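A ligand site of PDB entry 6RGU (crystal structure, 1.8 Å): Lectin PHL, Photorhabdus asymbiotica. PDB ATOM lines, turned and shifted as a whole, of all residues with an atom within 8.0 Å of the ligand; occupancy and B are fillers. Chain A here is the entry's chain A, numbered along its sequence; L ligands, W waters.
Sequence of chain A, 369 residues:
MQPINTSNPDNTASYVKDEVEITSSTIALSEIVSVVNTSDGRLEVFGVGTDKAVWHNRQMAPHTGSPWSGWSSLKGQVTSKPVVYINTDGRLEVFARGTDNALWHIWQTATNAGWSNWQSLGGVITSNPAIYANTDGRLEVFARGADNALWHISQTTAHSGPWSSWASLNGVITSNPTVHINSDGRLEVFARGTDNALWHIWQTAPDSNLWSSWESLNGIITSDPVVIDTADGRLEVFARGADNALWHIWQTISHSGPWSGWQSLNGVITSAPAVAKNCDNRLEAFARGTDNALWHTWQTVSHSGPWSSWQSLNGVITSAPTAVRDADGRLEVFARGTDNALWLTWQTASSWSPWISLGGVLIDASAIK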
ATOM      1  N   LYS A  52     -26.694  10.428 -16.755  1.00  0.00           N
ATOM      2  CA  LYS A  52     -25.462  10.324 -17.590  1.00  0.00           C
ATOM      3  C   LYS A  52     -24.309  11.127 -16.977  1.00  0.00           C
ATOM      4  O   LYS A  52     -23.306  11.372 -17.685  1.00  0.00           O
ATOM      5  CB  LYS A  52     -25.742  10.798 -19.026  1.00  0.00           C
ATOM      6  CG  LYS A  52     -26.886  10.076 -19.727  1.00  0.00           C
ATOM      7  CD  LYS A  52     -26.448   9.096 -20.792  1.00  0.00           C
ATOM      8  CE  LYS A  52     -25.755   9.762 -21.963  1.00  0.00           C
ATOM      9  NZ  LYS A  52     -26.643  10.695 -22.690  1.00  0.00           N
ATOM     10  N   ALA A  53     -24.424  11.527 -15.712  1.00  0.00           N
ATOM     11  CA  ALA A  53     -23.313  12.163 -14.973  1.00  0.00           C
ATOM     12  C   ALA A  53     -22.434  11.053 -14.400  1.00  0.00           C
ATOM     13  O   ALA A  53     -22.910   9.908 -14.242  1.00  0.00           O
ATOM     14  CB  ALA A  53     -23.820  13.100 -13.900  1.00  0.00           C
ATOM     15  N   VAL A  54     -21.186  11.387 -14.106  1.00  0.00           N
ATOM     16  CA  VAL A  54     -20.247  10.458 -13.418  1.00  0.00           C
ATOM     17  C   VAL A  54     -20.406  10.671 -11.924  1.00  0.00           C
ATOM     18  O   VAL A  54     -20.323  11.824 -11.486  1.00  0.00           O
ATOM     19  CB  VAL A  54     -18.797  10.699 -13.880  1.00  0.00           C
ATOM     20  CG1 VAL A  54     -17.810   9.890 -13.059  1.00  0.00           C
ATOM     21  CG2 VAL A  54     -18.638  10.392 -15.364  1.00  0.00           C
ATOM     22  N   LEU A  74     -19.714  14.017 -10.055  1.00  0.00           N
ATOM     23  CA  LEU A  74     -18.673  14.842 -10.707  1.00  0.00           C
ATOM     24  C   LEU A  74     -19.305  15.522 -11.927  1.00  0.00           C
ATOM     25  O   LEU A  74     -18.565  16.158 -12.666  1.00  0.00           O
ATOM     26  CB  LEU A  74     -17.498  13.952 -11.104  1.00  0.00           C
ATOM     27  CG  LEU A  74     -16.716  13.380  -9.936  1.00  0.00           C
ATOM     28  CD1 LEU A  74     -15.650  12.401 -10.429  1.00  0.00           C
ATOM     29  CD2 LEU A  74     -16.087  14.488  -9.109  1.00  0.00           C
ATOM     30  N   LYS A  75     -20.616  15.386 -12.102  1.00  0.00           N
ATOM     31  CA  LYS A  75     -21.381  16.002 -13.227  1.00  0.00           C
ATOM     32  C   LYS A  75     -20.828  15.449 -14.546  1.00  0.00           C
ATOM     33  O   LYS A  75     -20.466  14.255 -14.598  1.00  0.00           O
ATOM     34  CB  LYS A  75     -21.340  17.525 -13.108  1.00  0.00           C
ATOM     35  CG  LYS A  75     -21.794  18.072 -11.753  1.00  0.00           C
ATOM     36  CD  LYS A  75     -21.822  19.574 -11.649  1.00  0.00           C
ATOM     37  N   GLY A  76     -20.798  16.261 -15.597  1.00  0.00           N
ATOM     38  CA  GLY A  76     -20.525  15.801 -16.972  1.00  0.00           C
ATOM     39  C   GLY A  76     -21.705  15.055 -17.571  1.00  0.00           C
ATOM     40  O   GLY A  76     -22.667  14.741 -16.855  1.00  0.00           O
ATOM     41  N   GLN A  77     -21.632  14.803 -18.872  1.00  0.00           N
ATOM     42  CA  GLN A  77     -22.560  13.936 -19.620  1.00  0.00           C
ATOM     43  C   GLN A  77     -21.683  12.971 -20.424  1.00  0.00           C
ATOM     44  O   GLN A  77     -20.967  13.459 -21.301  1.00  0.00           O
ATOM     45  CB  GLN A  77     -23.468  14.790 -20.513  1.00  0.00           C
ATOM     46  CG  GLN A  77     -24.404  15.698 -19.724  1.00  0.00           C
ATOM     47  CD  GLN A  77     -25.518  14.906 -19.080  1.00  0.00           C
ATOM     48  OE1 GLN A  77     -26.527  14.578 -19.712  1.00  0.00           O
ATOM     49  NE2 GLN A  77     -25.349  14.605 -17.800  1.00  0.00           N
ATOM     50  N   VAL A  78     -21.688  11.698 -20.081  1.00  0.00           N
ATOM     51  CA  VAL A  78     -20.731  10.724 -20.679  1.00  0.00           C
ATOM     52  C   VAL A  78     -21.492   9.641 -21.436  1.00  0.00           C
ATOM     53  O   VAL A  78     -22.649   9.335 -21.068  1.00  0.00           O
ATOM     54  CB  VAL A  78     -19.788  10.135 -19.615  1.00  0.00           C
ATOM     55  CG1 VAL A  78     -19.033  11.240 -18.907  1.00  0.00           C
ATOM     56  CG2 VAL A  78     -20.497   9.227 -18.624  1.00  0.00           C
ATOM     57  N   THR A  79     -20.800   9.059 -22.429  1.00  0.00           N
ATOM     58  CA  THR A  79     -21.301   8.012 -23.342  1.00  0.00           C
ATOM     59  C   THR A  79     -20.293   6.863 -23.428  1.00  0.00           C
ATOM     60  O   THR A  79     -20.272   6.160 -24.455  1.00  0.00           O
ATOM     61  CB  THR A  79     -21.577   8.635 -24.712  1.00  0.00           C
ATOM     62  OG1 THR A  79     -20.328   9.140 -25.180  1.00  0.00           O
ATOM     63  CG2 THR A  79     -22.603   9.746 -24.655  1.00  0.00           C
ATOM     64  N   ALA A  96     -13.496   9.841 -19.933  1.00  0.00           N
ATOM     65  CA  ALA A  96     -14.799   9.382 -20.453  1.00  0.00           C
ATOM     66  C   ALA A  96     -15.058  10.028 -21.810  1.00  0.00           C
ATOM     67  O   ALA A  96     -14.625  11.162 -22.050  1.00  0.00           O
ATOM     68  CB  ALA A  96     -15.885   9.748 -19.483  1.00  0.00           C
ATOM     69  N   ARG A  97     -15.774   9.301 -22.668  1.00  0.00           N
ATOM     70  CA  ARG A  97     -16.340   9.888 -23.891  1.00  0.00           C
ATOM     71  C   ARG A  97     -17.496  10.827 -23.515  1.00  0.00           C
ATOM     72  O   ARG A  97     -18.299  10.434 -22.629  1.00  0.00           O
ATOM     73  CB  ARG A  97     -16.831   8.794 -24.828  1.00  0.00           C
ATOM     74  CG  ARG A  97     -17.112   9.317 -26.225  1.00  0.00           C
ATOM     75  CD  ARG A  97     -17.492   8.205 -27.160  1.00  0.00           C
ATOM     76  NE  ARG A  97     -18.725   7.528 -26.793  1.00  0.00           N
ATOM     77  CZ  ARG A  97     -19.346   6.642 -27.572  1.00  0.00           C
ATOM     78  NH1 ARG A  97     -18.842   6.336 -28.760  1.00  0.00           N
ATOM     79  NH2 ARG A  97     -20.454   6.054 -27.149  1.00  0.00           N
ATOM     80  N   GLY A  98     -17.594  11.961 -24.201  1.00  0.00           N
ATOM     81  CA  GLY A  98     -18.656  12.965 -24.006  1.00  0.00           C
ATOM     82  C   GLY A  98     -19.786  12.734 -25.000  1.00  0.00           C
ATOM     83  O   GLY A  98     -19.675  11.849 -25.836  1.00  0.00           O
ATOM     84  N   THR A  99     -20.851  13.534 -24.923  1.00  0.00           N
ATOM     85  CA  THR A  99     -22.034  13.388 -25.825  1.00  0.00           C
ATOM     86  C   THR A  99     -21.628  13.825 -27.235  1.00  0.00           C
ATOM     87  O   THR A  99     -22.354  13.454 -28.188  1.00  0.00           O
ATOM     88  CB  THR A  99     -23.245  14.106 -25.214  1.00  0.00           C
ATOM     89  OG1 THR A  99     -22.891  15.450 -24.961  1.00  0.00           O
ATOM     90  CG2 THR A  99     -23.694  13.472 -23.919  1.00  0.00           C
ATOM     91  N   ASP A 100     -20.495  14.542 -27.374  1.00  0.00           N
ATOM     92  CA  ASP A 100     -19.925  14.989 -28.668  1.00  0.00           C
ATOM     93  C   ASP A 100     -18.932  13.945 -29.227  1.00  0.00           C
ATOM     94  O   ASP A 100     -18.325  14.247 -30.256  1.00  0.00           O
ATOM     95  CB  ASP A 100     -19.247  16.350 -28.538  1.00  0.00           C
ATOM     96  CG  ASP A 100     -18.099  16.406 -27.537  1.00  0.00           C
ATOM     97  OD1 ASP A 100     -17.849  15.368 -26.873  1.00  0.00           O
ATOM     98  OD2 ASP A 100     -17.471  17.472 -27.417  1.00  0.00           O
ATOM     99  N   ASN A 101     -18.807  12.782 -28.565  1.00  0.00           N
ATOM    100  CA  ASN A 101     -17.867  11.668 -28.878  1.00  0.00           C
ATOM    101  C   ASN A 101     -16.393  12.115 -28.765  1.00  0.00           C
ATOM    102  O   ASN A 101     -15.523  11.350 -29.203  1.00  0.00           O
ATOM    103  CB  ASN A 101     -18.142  11.027 -30.241  1.00  0.00           C
ATOM    104  CG  ASN A 101     -19.361  10.141 -30.231  1.00  0.00           C
ATOM    105  OD1 ASN A 101     -19.734   9.617 -29.183  1.00  0.00           O
ATOM    106  ND2 ASN A 101     -19.998   9.978 -31.381  1.00  0.00           N
ATOM    107  N   ALA A 102     -16.105  13.268 -28.160  1.00  0.00           N
ATOM    108  CA  ALA A 102     -14.722  13.656 -27.808  1.00  0.00           C
ATOM    109  C   ALA A 102     -14.300  12.908 -26.541  1.00  0.00           C
ATOM    110  O   ALA A 102     -15.154  12.385 -25.792  1.00  0.00           O
ATOM    111  CB  ALA A 102     -14.610  15.142 -27.616  1.00  0.00           C
ATOM    112  N   LEU A 103     -12.997  12.852 -26.305  1.00  0.00           N
ATOM    113  CA  LEU A 103     -12.461  12.336 -25.021  1.00  0.00           C
ATOM    114  C   LEU A 103     -12.480  13.511 -24.055  1.00  0.00           C
ATOM    115  O   LEU A 103     -11.924  14.579 -24.394  1.00  0.00           O
ATOM    116  CB  LEU A 103     -11.048  11.801 -25.213  1.00  0.00           C
ATOM    117  CG  LEU A 103     -10.350  11.364 -23.921  1.00  0.00           C
ATOM    118  CD1 LEU A 103     -11.058  10.161 -23.310  1.00  0.00           C
ATOM    119  CD2 LEU A 103      -8.890  11.045 -24.175  1.00  0.00           C
ATOM    120  N   TRP A 104     -13.112  13.329 -22.902  1.00  0.00           N
ATOM    121  CA  TRP A 104     -13.117  14.342 -21.825  1.00  0.00           C
ATOM    122  C   TRP A 104     -12.336  13.781 -20.631  1.00  0.00           C
ATOM    123  O   TRP A 104     -12.226  12.554 -20.513  1.00  0.00           O
ATOM    124  CB  TRP A 104     -14.550  14.706 -21.458  1.00  0.00           C
ATOM    125  CG  TRP A 104     -15.239  15.490 -22.524  1.00  0.00           C
ATOM    126  CD1 TRP A 104     -15.779  15.020 -23.691  1.00  0.00           C
ATOM    127  CD2 TRP A 104     -15.454  16.910 -22.536  1.00  0.00           C
ATOM    128  NE1 TRP A 104     -16.331  16.046 -24.411  1.00  0.00           N
ATOM    129  CE2 TRP A 104     -16.146  17.214 -23.731  1.00  0.00           C
ATOM    130  CE3 TRP A 104     -15.165  17.950 -21.641  1.00  0.00           C
ATOM    131  CZ2 TRP A 104     -16.528  18.517 -24.051  1.00  0.00           C
ATOM    132  CZ3 TRP A 104     -15.553  19.232 -21.960  1.00  0.00           C
ATOM    133  CH2 TRP A 104     -16.222  19.515 -23.145  1.00  0.00           C
ATOM    134  N   HIS A 105     -11.864  14.651 -19.757  1.00  0.00           N
ATOM    135  CA  HIS A 105     -11.188  14.218 -18.514  1.00  0.00           C
ATOM    136  C   HIS A 105     -11.406  15.268 -17.428  1.00  0.00           C
ATOM    137  O   HIS A 105     -11.740  16.424 -17.744  1.00  0.00           O
ATOM    138  CB  HIS A 105      -9.716  13.872 -18.764  1.00  0.00           C
ATOM    139  CG  HIS A 105      -8.841  15.010 -19.164  1.00  0.00           C
ATOM    140  ND1 HIS A 105      -7.556  15.128 -18.673  1.00  0.00           N
ATOM    141  CD2 HIS A 105      -9.038  16.073 -19.969  1.00  0.00           C
ATOM    142  CE1 HIS A 105      -6.987  16.219 -19.176  1.00  0.00           C
ATOM    143  NE2 HIS A 105      -7.884  16.820 -19.981  1.00  0.00           N
ATOM    144  N   ILE A 106     -11.220  14.821 -16.207  1.00  0.00           N
ATOM    145  CA  ILE A 106     -11.374  15.620 -14.963  1.00  0.00           C
ATOM    146  C   ILE A 106     -10.371  15.015 -13.975  1.00  0.00           C
ATOM    147  O   ILE A 106     -10.163  13.784 -14.008  1.00  0.00           O
ATOM    148  CB  ILE A 106     -12.828  15.580 -14.473  1.00  0.00           C
ATOM    149  CG1 ILE A 106     -13.075  16.541 -13.318  1.00  0.00           C
ATOM    150  CG2 ILE A 106     -13.234  14.157 -14.120  1.00  0.00           C
ATOM    151  CD1 ILE A 106     -14.532  16.580 -12.855  1.00  0.00           C
ATOM    152  N   ASN A 117     -12.675  21.193 -13.391  1.00  0.00           N
ATOM    153  CA  ASN A 117     -13.843  21.028 -14.283  1.00  0.00           C
ATOM    154  C   ASN A 117     -13.509  19.966 -15.330  1.00  0.00           C
ATOM    155  O   ASN A 117     -12.292  19.723 -15.570  1.00  0.00           O
ATOM    156  CB  ASN A 117     -14.247  22.344 -14.957  1.00  0.00           C
ATOM    157  CG  ASN A 117     -14.710  23.379 -13.956  1.00  0.00           C
ATOM    158  OD1 ASN A 117     -15.312  23.050 -12.947  1.00  0.00           O
ATOM    159  ND2 ASN A 117     -14.393  24.634 -14.230  1.00  0.00           N
ATOM    160  N   TRP A 118     -14.533  19.372 -15.930  1.00  0.00           N
ATOM    161  CA  TRP A 118     -14.375  18.536 -17.142  1.00  0.00           C
ATOM    162  C   TRP A 118     -13.739  19.395 -18.237  1.00  0.00           C
ATOM    163  O   TRP A 118     -14.198  20.547 -18.447  1.00  0.00           O
ATOM    164  CB  TRP A 118     -15.718  17.964 -17.582  1.00  0.00           C
ATOM    165  CG  TRP A 118     -16.219  16.826 -16.747  1.00  0.00           C
ATOM    166  CD1 TRP A 118     -17.148  16.896 -15.751  1.00  0.00           C
ATOM    167  CD2 TRP A 118     -15.867  15.437 -16.861  1.00  0.00           C
ATOM    168  NE1 TRP A 118     -17.412  15.657 -15.259  1.00  0.00           N
ATOM    169  CE2 TRP A 118     -16.640  14.741 -15.911  1.00  0.00           C
ATOM    170  CE3 TRP A 118     -14.995  14.713 -17.679  1.00  0.00           C
ATOM    171  CZ2 TRP A 118     -16.556  13.356 -15.747  1.00  0.00           C
ATOM    172  CZ3 TRP A 118     -14.904  13.349 -17.517  1.00  0.00           C
ATOM    173  CH2 TRP A 118     -15.689  12.680 -16.571  1.00  0.00           C
ATOM    174  N   GLN A 119     -12.723  18.864 -18.912  1.00  0.00           N
ATOM    175  CA  GLN A 119     -12.081  19.538 -20.073  1.00  0.00           C
ATOM    176  C   GLN A 119     -11.974  18.516 -21.212  1.00  0.00           C
ATOM    177  O   GLN A 119     -11.853  17.306 -20.932  1.00  0.00           O
ATOM    178  CB  GLN A 119     -10.727  20.127 -19.678  1.00  0.00           C
ATOM    179  CG  GLN A 119     -10.803  21.165 -18.568  1.00  0.00           C
ATOM    180  CD  GLN A 119     -11.603  22.395 -18.944  1.00  0.00           C
ATOM    181  OE1 GLN A 119     -11.815  22.684 -20.120  1.00  0.00           O
ATOM    182  NE2 GLN A 119     -12.041  23.144 -17.941  1.00  0.00           N
ATOM    183  N   SER A 120     -12.044  19.013 -22.460  1.00  0.00           N
ATOM    184  CA  SER A 120     -12.027  18.194 -23.684  1.00  0.00           C
ATOM    185  C   SER A 120     -10.581  17.983 -24.156  1.00  0.00           C
ATOM    186  O   SER A 120      -9.814  18.958 -24.217  1.00  0.00           O
ATOM    187  CB  SER A 120     -12.868  18.830 -24.758  1.00  0.00           C
ATOM    188  OG  SER A 120     -12.848  18.025 -25.910  1.00  0.00           O
HETATM  189  O1  LIG L   1     -20.750  18.766 -25.213  1.00  0.00           O
HETATM  190  C1  LIG L   1     -21.002  17.682 -24.310  1.00  0.00           C
HETATM  191  C2  LIG L   1     -20.035  17.824 -23.141  1.00  0.00           C
HETATM  192  O2  LIG L   1     -20.280  19.095 -22.555  1.00  0.00           O
HETATM  193  C3  LIG L   1     -20.230  16.754 -22.097  1.00  0.00           C
HETATM  194  O3  LIG L   1     -20.069  15.448 -22.631  1.00  0.00           O
HETATM  195  C4  LIG L   1     -19.232  17.000 -20.981  1.00  0.00           C
HETATM  196  O4  LIG L   1     -19.301  15.943 -20.039  1.00  0.00           O
HETATM  197  C5  LIG L   1     -18.058  15.278 -19.908  1.00  0.00           C
HETATM  198  C6  LIG L   1     -19.533  18.354 -20.348  1.00  0.00           C
HETATM  199  O5  LIG L   1     -18.585  18.601 -19.312  1.00  0.00           O
HETATM  200  C7  LIG L   1     -19.416  19.412 -21.452  1.00  0.00           C
HETATM  201  O6  LIG L   1     -19.736  20.719 -20.984  1.00  0.00           O
HETATM  202  O   HOH W   1     -19.907  19.342 -16.713  1.00  0.00           O
HETATM  203  O   HOH W   2     -16.802  21.399 -18.981  1.00  0.00           O
HETATM  204  O   HOH W   3     -22.612  17.703 -27.304  1.00  0.00           O
HETATM  205  O   HOH W   4     -18.575  22.475 -22.939  1.00  0.00           O
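N of Gln 77 is in hydrogen-bond range of O4 of the ligand (2.8 Å).
The backbone carbonyl oxygen of Gln 77 is in hydrogen-bond range of an oxygen (O3) of the ligand, 2.6 Å away.
The backbone NH (N) of Thr 99 lies within hydrogen-bond range of an oxygen (O3) of the ligand (3.1 Å).
O of Gly 98 is in hydrogen-bond range of OG1 of Thr 79.
NE1 of Trp 118 lies within hydrogen-bond range of O of Lys 75 (3.4 Å).
O of Leu 74 lies within hydrogen-bond range of NE1 of Trp 118.
The side-chain carboxylate (OD1) of Asp 100 sits at hydrogen-bond distance from the indole nitrogen (NE1) of Trp 104 (3.0 Å).
The backbone NH (N) of Trp 104 lies within hydrogen-bond range of the backbone carbonyl oxygen (O) of Ala 96.
Gly 76 touches the ligand (CA to O4, 3.3 Å).
CA of Gly 98 touches O3 of the ligand (3.2 Å).
CH2 of Trp 104 touches C7 of the ligand, 3.6 Å away.
Trp 118 touches the ligand (CB to O5, 3.4 Å).
Hydrophobic or aromatic side chains that line the ligand: Trp 104 and Trp 118.
Six residues have an atom within 4 Å of the ligand: Gly 76, Gln 77, Gly 98, Thr 99, Trp 104 and Trp 118.
Water W3 bridges O1 of the ligand (3.0 Å) and OG1 of Thr 99 (3.3 Å).
Water W1 lies within hydrogen-bond range of O5 of the ligand (3.0 Å) and N of Gly 76 (3.4 Å).
Water W2 lies within hydrogen-bond range of O of Trp 118 (2.8 Å) and O5 of the ligand (3.3 Å).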
